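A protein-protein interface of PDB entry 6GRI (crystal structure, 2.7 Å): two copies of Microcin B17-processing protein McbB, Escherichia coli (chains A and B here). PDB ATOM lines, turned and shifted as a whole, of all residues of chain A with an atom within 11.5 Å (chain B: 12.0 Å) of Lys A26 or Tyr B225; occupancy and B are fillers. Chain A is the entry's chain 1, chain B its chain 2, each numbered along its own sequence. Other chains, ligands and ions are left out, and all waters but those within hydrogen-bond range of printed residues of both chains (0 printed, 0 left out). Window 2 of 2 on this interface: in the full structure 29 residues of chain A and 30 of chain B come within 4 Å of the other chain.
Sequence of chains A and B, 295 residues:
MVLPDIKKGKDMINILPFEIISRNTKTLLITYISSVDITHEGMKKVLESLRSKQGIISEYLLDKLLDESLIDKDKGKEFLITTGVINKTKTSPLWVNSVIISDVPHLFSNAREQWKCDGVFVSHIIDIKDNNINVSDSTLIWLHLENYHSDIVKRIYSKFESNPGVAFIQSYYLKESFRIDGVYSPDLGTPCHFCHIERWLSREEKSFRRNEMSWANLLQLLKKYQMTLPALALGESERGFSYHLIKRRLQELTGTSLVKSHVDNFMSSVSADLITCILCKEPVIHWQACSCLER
The backbone carbonyl oxygen (O) of Ser A35 lies close to the side-chain sulfur (SD) of Met B213, 3.1 Å away.
N of Glu A19 sits at hydrogen-bond distance from O of Ile A30 (2.9 Å).
O of Ile A21 is in hydrogen-bond range of N of Leu A28, 3.1 Å away.
OG of Ser A22 sits at hydrogen-bond distance from O of Lys A26, 3.2 Å away.
OG1 of Thr A27 is in hydrogen-bond range of OG of Ser A22.
O of Tyr B148 lies within hydrogen-bond range of N of Leu B229, at 2.9 Å.
N of Met B227 lies within hydrogen-bond range of O of Leu B222, 2.8 Å away.
Pro B230 touches Glu A19 (CG to CG, 3.9 Å).
CD2 of Leu B222 touches CD1 of Ile A21, at 3.8 Å.
Met B227 touches Ile A21 (CE to C, 3.5 Å).
Thr B228 touches Ile A21.
Arg A23 touches Tyr B225.
Arg A23 touches Gln B226 (CD to O, 2.9 Å).
Tyr B225 touches Lys A26.
Leu A28 touches Met B213.
Ile A30 touches Leu B229 (CD1 to CD1, 3.7 Å).
Ser A35 touches Leu B218 (OG to CD2, 3.4 Å).
Of chain B, only Tyr B225 (3.9 Å) comes within 4 Å of Lys A26.
Of chain A, only Arg A23 and Lys A26 come within 4 Å of Tyr B225.
Ser A22 touches just one residue of chain B: Met B227.
Of chain B, only Tyr B225, Gln B226 and Met B227 come within 4 Å of Arg A23.
Of the printed residues of chain B, Leu A28 touches Met B213 and Leu B218.
No residue of chain A comes within 4 Å of Leu B221.
No residue of chain A comes within 4 Å of Lys B223.
No residue of chain A comes within 4 Å of Lys B224.
Gln B226 touches just one residue of chain A: Arg A23 (2.9 Å).
Of chain A, only Ile A21, Ser A22 and Arg A23 come within 4 Å of Met B227.
Of the printed residues of chain A, Met B213 touches Leu A28 and Ser A35.
Of the printed residues of chain A, Leu B222 touches Ile A21.
His B149 touches none of the printed residues of chain A.
The nearest residue of chain B that does not touch Lys A26 is Met B227 (4.9 Å).
The nearest residue of chain A that does not touch Tyr B225 is Asn A24 (6.4 Å).
The nearest printed residue of chain B that does not touch Glu A19 is Leu B229 (7.2 Å).
Printed residues of chain B that touch a printed residue of chain A: Met B213, Leu B218, Leu B222, Tyr B225, Gln B226, Met B227, Thr B228, Leu B229 and Pro B230.
Hydrophobic or aromatic side chains of chain B within 4 Å of the printed part of chain A: Met B213, Leu B218, Leu B222, Tyr B225, Met B227, Leu B229 and Pro B230.
Along chain B the printed residues that touch a printed residue of chain A span positions 213 to 230.
Printed residues of chain A that touch a printed residue of chain B: Glu A19, Ile A21, Ser A22, Arg A23, Lys A26, Leu A28, Ile A30 and Ser A35.
Along chain A the printed residues that touch a printed residue of chain B span positions 19 to 35.
Among the printed residues, no Asp or Glu carboxylate lies within 4 Å of a Lys or Arg side-chain nitrogen of the other chain.
No position is printed for both chains.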
ATOM      1  N   GLU A  19     -10.449  26.757  16.233  1.00  0.00           N
ATOM      2  CA  GLU A  19      -9.090  26.620  16.700  1.00  0.00           C
ATOM      3  C   GLU A  19      -8.346  25.694  15.758  1.00  0.00           C
ATOM      4  O   GLU A  19      -8.937  24.872  15.053  1.00  0.00           O
ATOM      5  CB  GLU A  19      -9.056  26.075  18.126  1.00  0.00           C
ATOM      6  CG  GLU A  19      -9.706  26.978  19.169  1.00  0.00           C
ATOM      7  CD  GLU A  19      -9.007  28.315  19.327  1.00  0.00           C
ATOM      8  OE1 GLU A  19      -7.770  28.377  19.153  1.00  0.00           O
ATOM      9  OE2 GLU A  19      -9.710  29.306  19.623  1.00  0.00           O
ATOM     10  N   ILE A  20      -7.038  25.886  15.734  1.00  0.00           N
ATOM     11  CA  ILE A  20      -6.123  25.034  15.010  1.00  0.00           C
ATOM     12  C   ILE A  20      -5.042  24.691  16.032  1.00  0.00           C
ATOM     13  O   ILE A  20      -4.428  25.580  16.629  1.00  0.00           O
ATOM     14  CB  ILE A  20      -5.595  25.727  13.726  1.00  0.00           C
ATOM     15  CG1 ILE A  20      -4.880  24.715  12.827  1.00  0.00           C
ATOM     16  CG2 ILE A  20      -4.717  26.942  14.023  1.00  0.00           C
ATOM     17  CD1 ILE A  20      -5.822  23.950  11.923  1.00  0.00           C
ATOM     18  N   ILE A  21      -4.865  23.399  16.281  1.00  0.00           N
ATOM     19  CA  ILE A  21      -3.928  22.930  17.301  1.00  0.00           C
ATOM     20  C   ILE A  21      -3.048  21.833  16.710  1.00  0.00           C
ATOM     21  O   ILE A  21      -3.526  20.988  15.947  1.00  0.00           O
ATOM     22  CB  ILE A  21      -4.653  22.448  18.576  1.00  0.00           C
ATOM     23  CG1 ILE A  21      -5.913  21.648  18.223  1.00  0.00           C
ATOM     24  CG2 ILE A  21      -5.018  23.640  19.446  1.00  0.00           C
ATOM     25  CD1 ILE A  21      -6.476  20.842  19.371  1.00  0.00           C
ATOM     26  N   SER A  22      -1.757  21.881  17.044  1.00  0.00           N
ATOM     27  CA  SER A  22      -0.783  20.891  16.589  1.00  0.00           C
ATOM     28  C   SER A  22       0.258  20.632  17.673  1.00  0.00           C
ATOM     29  O   SER A  22       0.692  21.559  18.364  1.00  0.00           O
ATOM     30  CB  SER A  22      -0.113  21.349  15.298  1.00  0.00           C
ATOM     31  OG  SER A  22      -1.019  21.253  14.212  1.00  0.00           O
ATOM     32  N   ARG A  23       0.593  19.354  17.852  1.00  0.00           N
ATOM     33  CA  ARG A  23       1.798  18.934  18.563  1.00  0.00           C
ATOM     34  C   ARG A  23       2.513  17.992  17.598  1.00  0.00           C
ATOM     35  O   ARG A  23       1.923  16.995  17.163  1.00  0.00           O
ATOM     36  CB  ARG A  23       1.472  18.233  19.897  1.00  0.00           C
ATOM     37  CG  ARG A  23       2.639  18.197  20.879  1.00  0.00           C
ATOM     38  CD  ARG A  23       2.406  17.254  22.047  1.00  0.00           C
ATOM     39  N   ASN A  24       3.748  18.350  17.232  1.00  0.00           N
ATOM     40  CA  ASN A  24       4.608  17.545  16.359  1.00  0.00           C
ATOM     41  C   ASN A  24       3.927  17.110  15.045  1.00  0.00           C
ATOM     42  O   ASN A  24       3.912  17.878  14.076  1.00  0.00           O
ATOM     43  CB  ASN A  24       5.173  16.338  17.131  1.00  0.00           C
ATOM     44  N   THR A  25       3.334  15.909  15.039  1.00  0.00           N
ATOM     45  CA  THR A  25       2.877  15.242  13.809  1.00  0.00           C
ATOM     46  C   THR A  25       1.459  15.638  13.379  1.00  0.00           C
ATOM     47  O   THR A  25       1.246  16.029  12.228  1.00  0.00           O
ATOM     48  CB  THR A  25       2.919  13.709  13.960  1.00  0.00           C
ATOM     49  N   LYS A  26       0.503  15.532  14.303  1.00  0.00           N
ATOM     50  CA  LYS A  26      -0.919  15.719  13.988  1.00  0.00           C
ATOM     51  C   LYS A  26      -1.342  17.194  13.961  1.00  0.00           C
ATOM     52  O   LYS A  26      -0.724  18.043  14.616  1.00  0.00           O
ATOM     53  CB  LYS A  26      -1.791  14.944  14.984  1.00  0.00           C
ATOM     54  N   THR A  27      -2.404  17.467  13.199  1.00  0.00           N
ATOM     55  CA  THR A  27      -3.016  18.798  13.078  1.00  0.00           C
ATOM     56  C   THR A  27      -4.545  18.675  13.070  1.00  0.00           C
ATOM     57  O   THR A  27      -5.099  17.977  12.217  1.00  0.00           O
ATOM     58  CB  THR A  27      -2.560  19.483  11.771  1.00  0.00           C
ATOM     59  OG1 THR A  27      -1.144  19.691  11.815  1.00  0.00           O
ATOM     60  CG2 THR A  27      -3.257  20.823  11.552  1.00  0.00           C
ATOM     61  N   LEU A  28      -5.218  19.358  14.001  1.00  0.00           N
ATOM     62  CA  LEU A  28      -6.681  19.300  14.118  1.00  0.00           C
ATOM     63  C   LEU A  28      -7.338  20.684  14.047  1.00  0.00           C
ATOM     64  O   LEU A  28      -7.006  21.578  14.835  1.00  0.00           O
ATOM     65  CB  LEU A  28      -7.085  18.621  15.435  1.00  0.00           C
ATOM     66  CG  LEU A  28      -6.766  17.131  15.624  1.00  0.00           C
ATOM     67  CD1 LEU A  28      -7.182  16.715  17.028  1.00  0.00           C
ATOM     68  CD2 LEU A  28      -7.431  16.239  14.573  1.00  0.00           C
ATOM     69  N   LEU A  29      -8.268  20.835  13.100  1.00  0.00           N
ATOM     70  CA  LEU A  29      -9.187  21.977  13.052  1.00  0.00           C
ATOM     71  C   LEU A  29     -10.397  21.621  13.891  1.00  0.00           C
ATOM     72  O   LEU A  29     -11.009  20.583  13.654  1.00  0.00           O
ATOM     73  CB  LEU A  29      -9.646  22.265  11.614  1.00  0.00           C
ATOM     74  CG  LEU A  29     -10.834  23.225  11.409  1.00  0.00           C
ATOM     75  CD1 LEU A  29     -10.415  24.664  11.658  1.00  0.00           C
ATOM     76  CD2 LEU A  29     -11.453  23.084  10.024  1.00  0.00           C
ATOM     77  N   ILE A  30     -10.750  22.492  14.840  1.00  0.00           N
ATOM     78  CA  ILE A  30     -11.932  22.321  15.691  1.00  0.00           C
ATOM     79  C   ILE A  30     -12.830  23.549  15.504  1.00  0.00           C
ATOM     80  O   ILE A  30     -12.435  24.664  15.841  1.00  0.00           O
ATOM     81  CB  ILE A  30     -11.525  22.130  17.169  1.00  0.00           C
ATOM     82  CG1 ILE A  30     -10.636  20.887  17.305  1.00  0.00           C
ATOM     83  CG2 ILE A  30     -12.741  21.958  18.067  1.00  0.00           C
ATOM     84  CD1 ILE A  30     -10.224  20.544  18.725  1.00  0.00           C
ATOM     85  N   SER A  35     -14.759  18.711  13.253  1.00  0.00           N
ATOM     86  CA  SER A  35     -13.384  18.480  13.690  1.00  0.00           C
ATOM     87  C   SER A  35     -12.666  17.708  12.585  1.00  0.00           C
ATOM     88  O   SER A  35     -13.007  16.540  12.341  1.00  0.00           O
ATOM     89  CB  SER A  35     -13.369  17.669  14.983  1.00  0.00           C
ATOM     90  OG  SER A  35     -14.232  18.257  15.936  1.00  0.00           O
ATOM     91  N   VAL A  36     -11.697  18.348  11.913  1.00  0.00           N
ATOM     92  CA  VAL A  36     -11.077  17.768  10.704  1.00  0.00           C
ATOM     93  C   VAL A  36      -9.572  17.549  10.846  1.00  0.00           C
ATOM     94  O   VAL A  36      -8.846  18.443  11.279  1.00  0.00           O
ATOM     95  CB  VAL A  36     -11.368  18.620   9.446  1.00  0.00           C
ATOM     96  CG1 VAL A  36     -10.897  17.912   8.175  1.00  0.00           C
ATOM     97  CG2 VAL A  36     -12.854  18.920   9.360  1.00  0.00           C
ATOM     98  N   ASP A  37      -9.137  16.343  10.469  1.00  0.00           N
ATOM     99  CA  ASP A  37      -7.726  15.937  10.472  1.00  0.00           C
ATOM    100  C   ASP A  37      -7.065  16.435   9.171  1.00  0.00           C
ATOM    101  O   ASP A  37      -7.198  15.797   8.115  1.00  0.00           O
ATOM    102  CB  ASP A  37      -7.639  14.404  10.612  1.00  0.00           C
ATOM    103  CG  ASP A  37      -6.207  13.883  10.721  1.00  0.00           C
ATOM    104  OD1 ASP A  37      -5.413  14.076   9.776  1.00  0.00           O
ATOM    105  OD2 ASP A  37      -5.879  13.235  11.742  1.00  0.00           O
ATOM    106  N   ILE A  38      -6.347  17.562   9.264  1.00  0.00           N
ATOM    107  CA  ILE A  38      -5.805  18.259   8.090  1.00  0.00           C
ATOM    108  C   ILE A  38      -4.568  17.544   7.620  1.00  0.00           C
ATOM    109  O   ILE A  38      -3.582  17.485   8.344  1.00  0.00           O
ATOM    110  CB  ILE A  38      -5.399  19.727   8.389  1.00  0.00           C
ATOM    111  CG1 ILE A  38      -6.562  20.523   9.016  1.00  0.00           C
ATOM    112  CG2 ILE A  38      -4.873  20.409   7.125  1.00  0.00           C
ATOM    113  CD1 ILE A  38      -7.883  20.419   8.284  1.00  0.00           C
ATOM    114  N   THR A  39      -4.624  17.011   6.405  1.00  0.00           N
ATOM    115  CA  THR A  39      -3.483  16.328   5.791  1.00  0.00           C
ATOM    116  C   THR A  39      -2.740  17.200   4.758  1.00  0.00           C
ATOM    117  O   THR A  39      -1.717  16.787   4.228  1.00  0.00           O
ATOM    118  CB  THR A  39      -3.941  15.003   5.152  1.00  0.00           C
ATOM    119  OG1 THR A  39      -5.102  15.230   4.341  1.00  0.00           O
ATOM    120  CG2 THR A  39      -4.282  13.990   6.234  1.00  0.00           C
ATOM    121  N   HIS A  40      -3.251  18.401   4.489  1.00  0.00           N
ATOM    122  CA  HIS A  40      -2.610  19.363   3.582  1.00  0.00           C
ATOM    123  C   HIS A  40      -1.662  20.276   4.383  1.00  0.00           C
ATOM    124  O   HIS A  40      -1.748  20.349   5.604  1.00  0.00           O
ATOM    125  CB  HIS A  40      -3.685  20.182   2.846  1.00  0.00           C
ATOM    126  CG  HIS A  40      -3.312  20.557   1.446  1.00  0.00           C
ATOM    127  ND1 HIS A  40      -2.966  21.842   1.084  1.00  0.00           N
ATOM    128  CD2 HIS A  40      -3.238  19.814   0.316  1.00  0.00           C
ATOM    129  CE1 HIS A  40      -2.685  21.871  -0.207  1.00  0.00           C
ATOM    130  NE2 HIS A  40      -2.839  20.653  -0.696  1.00  0.00           N
ATOM    131  N   GLU A  41      -0.741  20.937   3.686  1.00  0.00           N
ATOM    132  CA  GLU A  41       0.227  21.867   4.297  1.00  0.00           C
ATOM    133  C   GLU A  41      -0.196  23.303   4.067  1.00  0.00           C
ATOM    134  O   GLU A  41      -0.019  24.155   4.939  1.00  0.00           O
ATOM    135  CB  GLU A  41       1.622  21.656   3.705  1.00  0.00           C
ATOM    136  N   LYS A  44      -3.384  24.163   6.366  1.00  0.00           N
ATOM    137  CA  LYS A  44      -2.947  24.536   7.715  1.00  0.00           C
ATOM    138  C   LYS A  44      -2.431  25.974   7.748  1.00  0.00           C
ATOM    139  O   LYS A  44      -2.687  26.699   8.715  1.00  0.00           O
ATOM    140  CB  LYS A  44      -1.858  23.586   8.230  1.00  0.00           C
ATOM    141  CG  LYS A  44      -1.501  23.811   9.696  1.00  0.00           C
ATOM    142  CD  LYS A  44      -0.267  23.028  10.114  1.00  0.00           C
ATOM    143  CE  LYS A  44       0.194  23.426  11.510  1.00  0.00           C
ATOM    144  NZ  LYS A  44       1.551  22.893  11.811  1.00  0.00           N
ATOM    145  N   LEU A  47      -5.459  28.235   7.405  1.00  0.00           N
ATOM    146  CA  LEU A  47      -6.162  28.173   8.697  1.00  0.00           C
ATOM    147  C   LEU A  47      -5.419  28.938   9.788  1.00  0.00           C
ATOM    148  O   LEU A  47      -6.039  29.648  10.588  1.00  0.00           O
ATOM    149  CB  LEU A  47      -6.428  26.721   9.130  1.00  0.00           C
ATOM    150  CG  LEU A  47      -7.554  26.008   8.369  1.00  0.00           C
ATOM    151  CD1 LEU A  47      -7.565  24.519   8.682  1.00  0.00           C
ATOM    152  CD2 LEU A  47      -8.913  26.616   8.680  1.00  0.00           C
ATOM    153  N   TYR B 148      -9.282  21.691  28.339  1.00  0.00           N
ATOM    154  CA  TYR B 148      -9.742  20.427  28.931  1.00  0.00           C
ATOM    155  C   TYR B 148      -8.882  19.233  28.543  1.00  0.00           C
ATOM    156  O   TYR B 148      -8.459  19.121  27.398  1.00  0.00           O
ATOM    157  CB  TYR B 148     -11.184  20.120  28.500  1.00  0.00           C
ATOM    158  CG  TYR B 148     -11.645  18.738  28.902  1.00  0.00           C
ATOM    159  CD1 TYR B 148     -11.787  18.399  30.250  1.00  0.00           C
ATOM    160  CD2 TYR B 148     -11.908  17.756  27.943  1.00  0.00           C
ATOM    161  CE1 TYR B 148     -12.195  17.132  30.636  1.00  0.00           C
ATOM    162  CE2 TYR B 148     -12.321  16.488  28.319  1.00  0.00           C
ATOM    163  CZ  TYR B 148     -12.458  16.181  29.666  1.00  0.00           C
ATOM    164  OH  TYR B 148     -12.855  14.925  30.051  1.00  0.00           O
ATOM    165  N   HIS B 149      -8.656  18.340  29.503  1.00  0.00           N
ATOM    166  CA  HIS B 149      -8.071  17.023  29.240  1.00  0.00           C
ATOM    167  C   HIS B 149      -8.453  16.081  30.381  1.00  0.00           C
ATOM    168  O   HIS B 149      -8.275  16.433  31.546  1.00  0.00           O
ATOM    169  CB  HIS B 149      -6.546  17.120  29.130  1.00  0.00           C
ATOM    170  CG  HIS B 149      -5.900  15.917  28.511  1.00  0.00           C
ATOM    171  ND1 HIS B 149      -5.793  14.708  29.165  1.00  0.00           N
ATOM    172  CD2 HIS B 149      -5.305  15.745  27.307  1.00  0.00           C
ATOM    173  CE1 HIS B 149      -5.179  13.838  28.386  1.00  0.00           C
ATOM    174  NE2 HIS B 149      -4.870  14.444  27.253  1.00  0.00           N
ATOM    175  N   SER B 150      -8.973  14.900  30.043  1.00  0.00           N
ATOM    176  CA  SER B 150      -9.332  13.855  31.026  1.00  0.00           C
ATOM    177  C   SER B 150      -8.264  13.601  32.108  1.00  0.00           C
ATOM    178  O   SER B 150      -8.590  13.497  33.293  1.00  0.00           O
ATOM    179  CB  SER B 150      -9.657  12.545  30.296  1.00  0.00           C
ATOM    180  OG  SER B 150      -8.916  12.431  29.092  1.00  0.00           O
ATOM    181  N   ASP B 151      -7.003  13.496  31.690  1.00  0.00           N
ATOM    182  CA  ASP B 151      -5.865  13.341  32.617  1.00  0.00           C
ATOM    183  C   ASP B 151      -5.646  14.502  33.615  1.00  0.00           C
ATOM    184  O   ASP B 151      -5.082  14.288  34.686  1.00  0.00           O
ATOM    185  CB  ASP B 151      -4.551  13.041  31.853  1.00  0.00           C
ATOM    186  CG  ASP B 151      -4.495  11.610  31.275  1.00  0.00           C
ATOM    187  OD1 ASP B 151      -5.234  10.716  31.747  1.00  0.00           O
ATOM    188  OD2 ASP B 151      -3.688  11.368  30.349  1.00  0.00           O
ATOM    189  N   MET B 213     -15.955  12.260  11.511  1.00  0.00           N
ATOM    190  CA  MET B 213     -15.179  12.358  12.743  1.00  0.00           C
ATOM    191  C   MET B 213     -16.093  12.680  13.931  1.00  0.00           C
ATOM    192  O   MET B 213     -16.603  13.799  14.042  1.00  0.00           O
ATOM    193  CB  MET B 213     -14.077  13.418  12.598  1.00  0.00           C
ATOM    194  CG  MET B 213     -13.249  13.657  13.859  1.00  0.00           C
ATOM    195  SD  MET B 213     -11.538  14.143  13.526  1.00  0.00           S
ATOM    196  CE  MET B 213     -11.008  14.694  15.143  1.00  0.00           C
ATOM    197  N   ALA B 216     -16.015  11.224  20.280  1.00  0.00           N
ATOM    198  CA  ALA B 216     -15.108  10.213  20.824  1.00  0.00           C
ATOM    199  C   ALA B 216     -13.882  10.050  19.923  1.00  0.00           C
ATOM    200  O   ALA B 216     -12.747   9.987  20.413  1.00  0.00           O
ATOM    201  CB  ALA B 216     -15.828   8.884  20.990  1.00  0.00           C
ATOM    202  N   ASN B 217     -14.117   9.991  18.609  1.00  0.00           N
ATOM    203  CA  ASN B 217     -13.030  10.008  17.627  1.00  0.00           C
ATOM    204  C   ASN B 217     -12.084  11.191  17.884  1.00  0.00           C
ATOM    205  O   ASN B 217     -10.858  11.023  17.856  1.00  0.00           O
ATOM    206  CB  ASN B 217     -13.581  10.056  16.198  1.00  0.00           C
ATOM    207  N   LEU B 218     -12.659  12.365  18.171  1.00  0.00           N
ATOM    208  CA  LEU B 218     -11.880  13.562  18.513  1.00  0.00           C
ATOM    209  C   LEU B 218     -11.150  13.484  19.851  1.00  0.00           C
ATOM    210  O   LEU B 218      -9.960  13.787  19.908  1.00  0.00           O
ATOM    211  CB  LEU B 218     -12.747  14.825  18.494  1.00  0.00           C
ATOM    212  CG  LEU B 218     -12.051  16.127  18.913  1.00  0.00           C
ATOM    213  CD1 LEU B 218     -10.862  16.463  18.019  1.00  0.00           C
ATOM    214  CD2 LEU B 218     -13.056  17.264  18.935  1.00  0.00           C
ATOM    215  N   LEU B 219     -11.855  13.130  20.924  1.00  0.00           N
ATOM    216  CA  LEU B 219     -11.211  12.979  22.238  1.00  0.00           C
ATOM    217  C   LEU B 219     -10.131  11.863  22.261  1.00  0.00           C
ATOM    218  O   LEU B 219      -9.176  11.937  23.052  1.00  0.00           O
ATOM    219  CB  LEU B 219     -12.252  12.736  23.336  1.00  0.00           C
ATOM    220  CG  LEU B 219     -13.210  13.867  23.711  1.00  0.00           C
ATOM    221  CD1 LEU B 219     -14.206  13.377  24.750  1.00  0.00           C
ATOM    222  CD2 LEU B 219     -12.470  15.080  24.247  1.00  0.00           C
ATOM    223  N   GLN B 220     -10.281  10.853  21.395  1.00  0.00           N
ATOM    224  CA  GLN B 220      -9.284   9.786  21.255  1.00  0.00           C
ATOM    225  C   GLN B 220      -7.980  10.306  20.634  1.00  0.00           C
ATOM    226  O   GLN B 220      -6.903  10.077  21.194  1.00  0.00           O
ATOM    227  CB  GLN B 220      -9.840   8.607  20.441  1.00  0.00           C
ATOM    228  N   LEU B 221      -8.076  10.999  19.495  1.00  0.00           N
ATOM    229  CA  LEU B 221      -6.891  11.606  18.841  1.00  0.00           C
ATOM    230  C   LEU B 221      -6.139  12.561  19.771  1.00  0.00           C
ATOM    231  O   LEU B 221      -4.916  12.477  19.886  1.00  0.00           O
ATOM    232  CB  LEU B 221      -7.270  12.351  17.554  1.00  0.00           C
ATOM    233  CG  LEU B 221      -7.419  11.484  16.304  1.00  0.00           C
ATOM    234  CD1 LEU B 221      -8.439  12.061  15.331  1.00  0.00           C
ATOM    235  CD2 LEU B 221      -6.067  11.313  15.635  1.00  0.00           C
ATOM    236  N   LEU B 222      -6.882  13.452  20.432  1.00  0.00           N
ATOM    237  CA  LEU B 222      -6.316  14.431  21.376  1.00  0.00           C
ATOM    238  C   LEU B 222      -5.424  13.765  22.419  1.00  0.00           C
ATOM    239  O   LEU B 222      -4.308  14.224  22.668  1.00  0.00           O
ATOM    240  CB  LEU B 222      -7.432  15.217  22.067  1.00  0.00           C
ATOM    241  CG  LEU B 222      -8.113  16.277  21.198  1.00  0.00           C
ATOM    242  CD1 LEU B 222      -9.505  16.591  21.722  1.00  0.00           C
ATOM    243  CD2 LEU B 222      -7.266  17.542  21.122  1.00  0.00           C
ATOM    244  N   LYS B 223      -5.919  12.675  23.005  1.00  0.00           N
ATOM    245  CA  LYS B 223      -5.119  11.847  23.905  1.00  0.00           C
ATOM    246  C   LYS B 223      -3.978  11.186  23.127  1.00  0.00           C
ATOM    247  O   LYS B 223      -2.799  11.342  23.484  1.00  0.00           O
ATOM    248  CB  LYS B 223      -5.988  10.780  24.585  1.00  0.00           C
ATOM    249  N   LYS B 224      -4.343  10.500  22.039  1.00  0.00           N
ATOM    250  CA  LYS B 224      -3.410   9.702  21.230  1.00  0.00           C
ATOM    251  C   LYS B 224      -2.251  10.479  20.592  1.00  0.00           C
ATOM    252  O   LYS B 224      -1.231   9.869  20.271  1.00  0.00           O
ATOM    253  CB  LYS B 224      -4.169   8.953  20.130  1.00  0.00           C
ATOM    254  N   TYR B 225      -2.418  11.789  20.385  1.00  0.00           N
ATOM    255  CA  TYR B 225      -1.336  12.663  19.913  1.00  0.00           C
ATOM    256  C   TYR B 225      -0.977  13.766  20.919  1.00  0.00           C
ATOM    257  O   TYR B 225      -0.376  14.772  20.536  1.00  0.00           O
ATOM    258  CB  TYR B 225      -1.700  13.271  18.556  1.00  0.00           C
ATOM    259  N   GLN B 226      -1.320  13.554  22.196  1.00  0.00           N
ATOM    260  CA  GLN B 226      -0.967  14.444  23.321  1.00  0.00           C
ATOM    261  C   GLN B 226      -1.282  15.927  23.100  1.00  0.00           C
ATOM    262  O   GLN B 226      -0.401  16.704  22.724  1.00  0.00           O
ATOM    263  CB  GLN B 226       0.521  14.293  23.681  1.00  0.00           C
ATOM    264  CG  GLN B 226       0.909  12.970  24.321  1.00  0.00           C
ATOM    265  CD  GLN B 226       2.324  12.999  24.874  1.00  0.00           C
ATOM    266  OE1 GLN B 226       2.611  13.727  25.823  1.00  0.00           O
ATOM    267  NE2 GLN B 226       3.214  12.212  24.279  1.00  0.00           N
ATOM    268  N   MET B 227      -2.538  16.310  23.317  1.00  0.00           N
ATOM    269  CA  MET B 227      -2.965  17.725  23.223  1.00  0.00           C
ATOM    270  C   MET B 227      -4.323  17.983  23.896  1.00  0.00           C
ATOM    271  O   MET B 227      -5.231  17.149  23.812  1.00  0.00           O
ATOM    272  CB  MET B 227      -2.986  18.207  21.760  1.00  0.00           C
ATOM    273  CG  MET B 227      -3.089  17.108  20.697  1.00  0.00           C
ATOM    274  SD  MET B 227      -3.360  17.676  19.004  1.00  0.00           S
ATOM    275  CE  MET B 227      -2.575  19.275  19.036  1.00  0.00           C
ATOM    276  N   THR B 228      -4.452  19.133  24.565  1.00  0.00           N
ATOM    277  CA  THR B 228      -5.709  19.496  25.236  1.00  0.00           C
ATOM    278  C   THR B 228      -6.770  20.022  24.253  1.00  0.00           C
ATOM    279  O   THR B 228      -6.468  20.335  23.101  1.00  0.00           O
ATOM    280  CB  THR B 228      -5.503  20.534  26.368  1.00  0.00           C
ATOM    281  OG1 THR B 228      -5.008  21.756  25.823  1.00  0.00           O
ATOM    282  CG2 THR B 228      -4.526  20.016  27.413  1.00  0.00           C
ATOM    283  N   LEU B 229      -8.015  20.088  24.731  1.00  0.00           N
ATOM    284  CA  LEU B 229      -9.148  20.564  23.955  1.00  0.00           C
ATOM    285  C   LEU B 229      -9.346  22.014  24.346  1.00  0.00           C
ATOM    286  O   LEU B 229      -9.718  22.297  25.489  1.00  0.00           O
ATOM    287  CB  LEU B 229     -10.408  19.754  24.270  1.00  0.00           C
ATOM    288  CG  LEU B 229     -11.705  20.194  23.582  1.00  0.00           C
ATOM    289  CD1 LEU B 229     -11.608  20.018  22.075  1.00  0.00           C
ATOM    290  CD2 LEU B 229     -12.890  19.419  24.135  1.00  0.00           C
ATOM    291  N   PRO B 230      -9.090  22.945  23.415  1.00  0.00           N
ATOM    292  CA  PRO B 230      -9.283  24.338  23.768  1.00  0.00           C
ATOM    293  C   PRO B 230     -10.748  24.767  23.684  1.00  0.00           C
ATOM    294  O   PRO B 230     -11.553  24.181  22.957  1.00  0.00           O
ATOM    295  CB  PRO B 230      -8.438  25.077  22.731  1.00  0.00           C
ATOM    296  CG  PRO B 230      -8.431  24.189  21.541  1.00  0.00           C
ATOM    297  CD  PRO B 230      -8.666  22.784  22.012  1.00  0.00           C
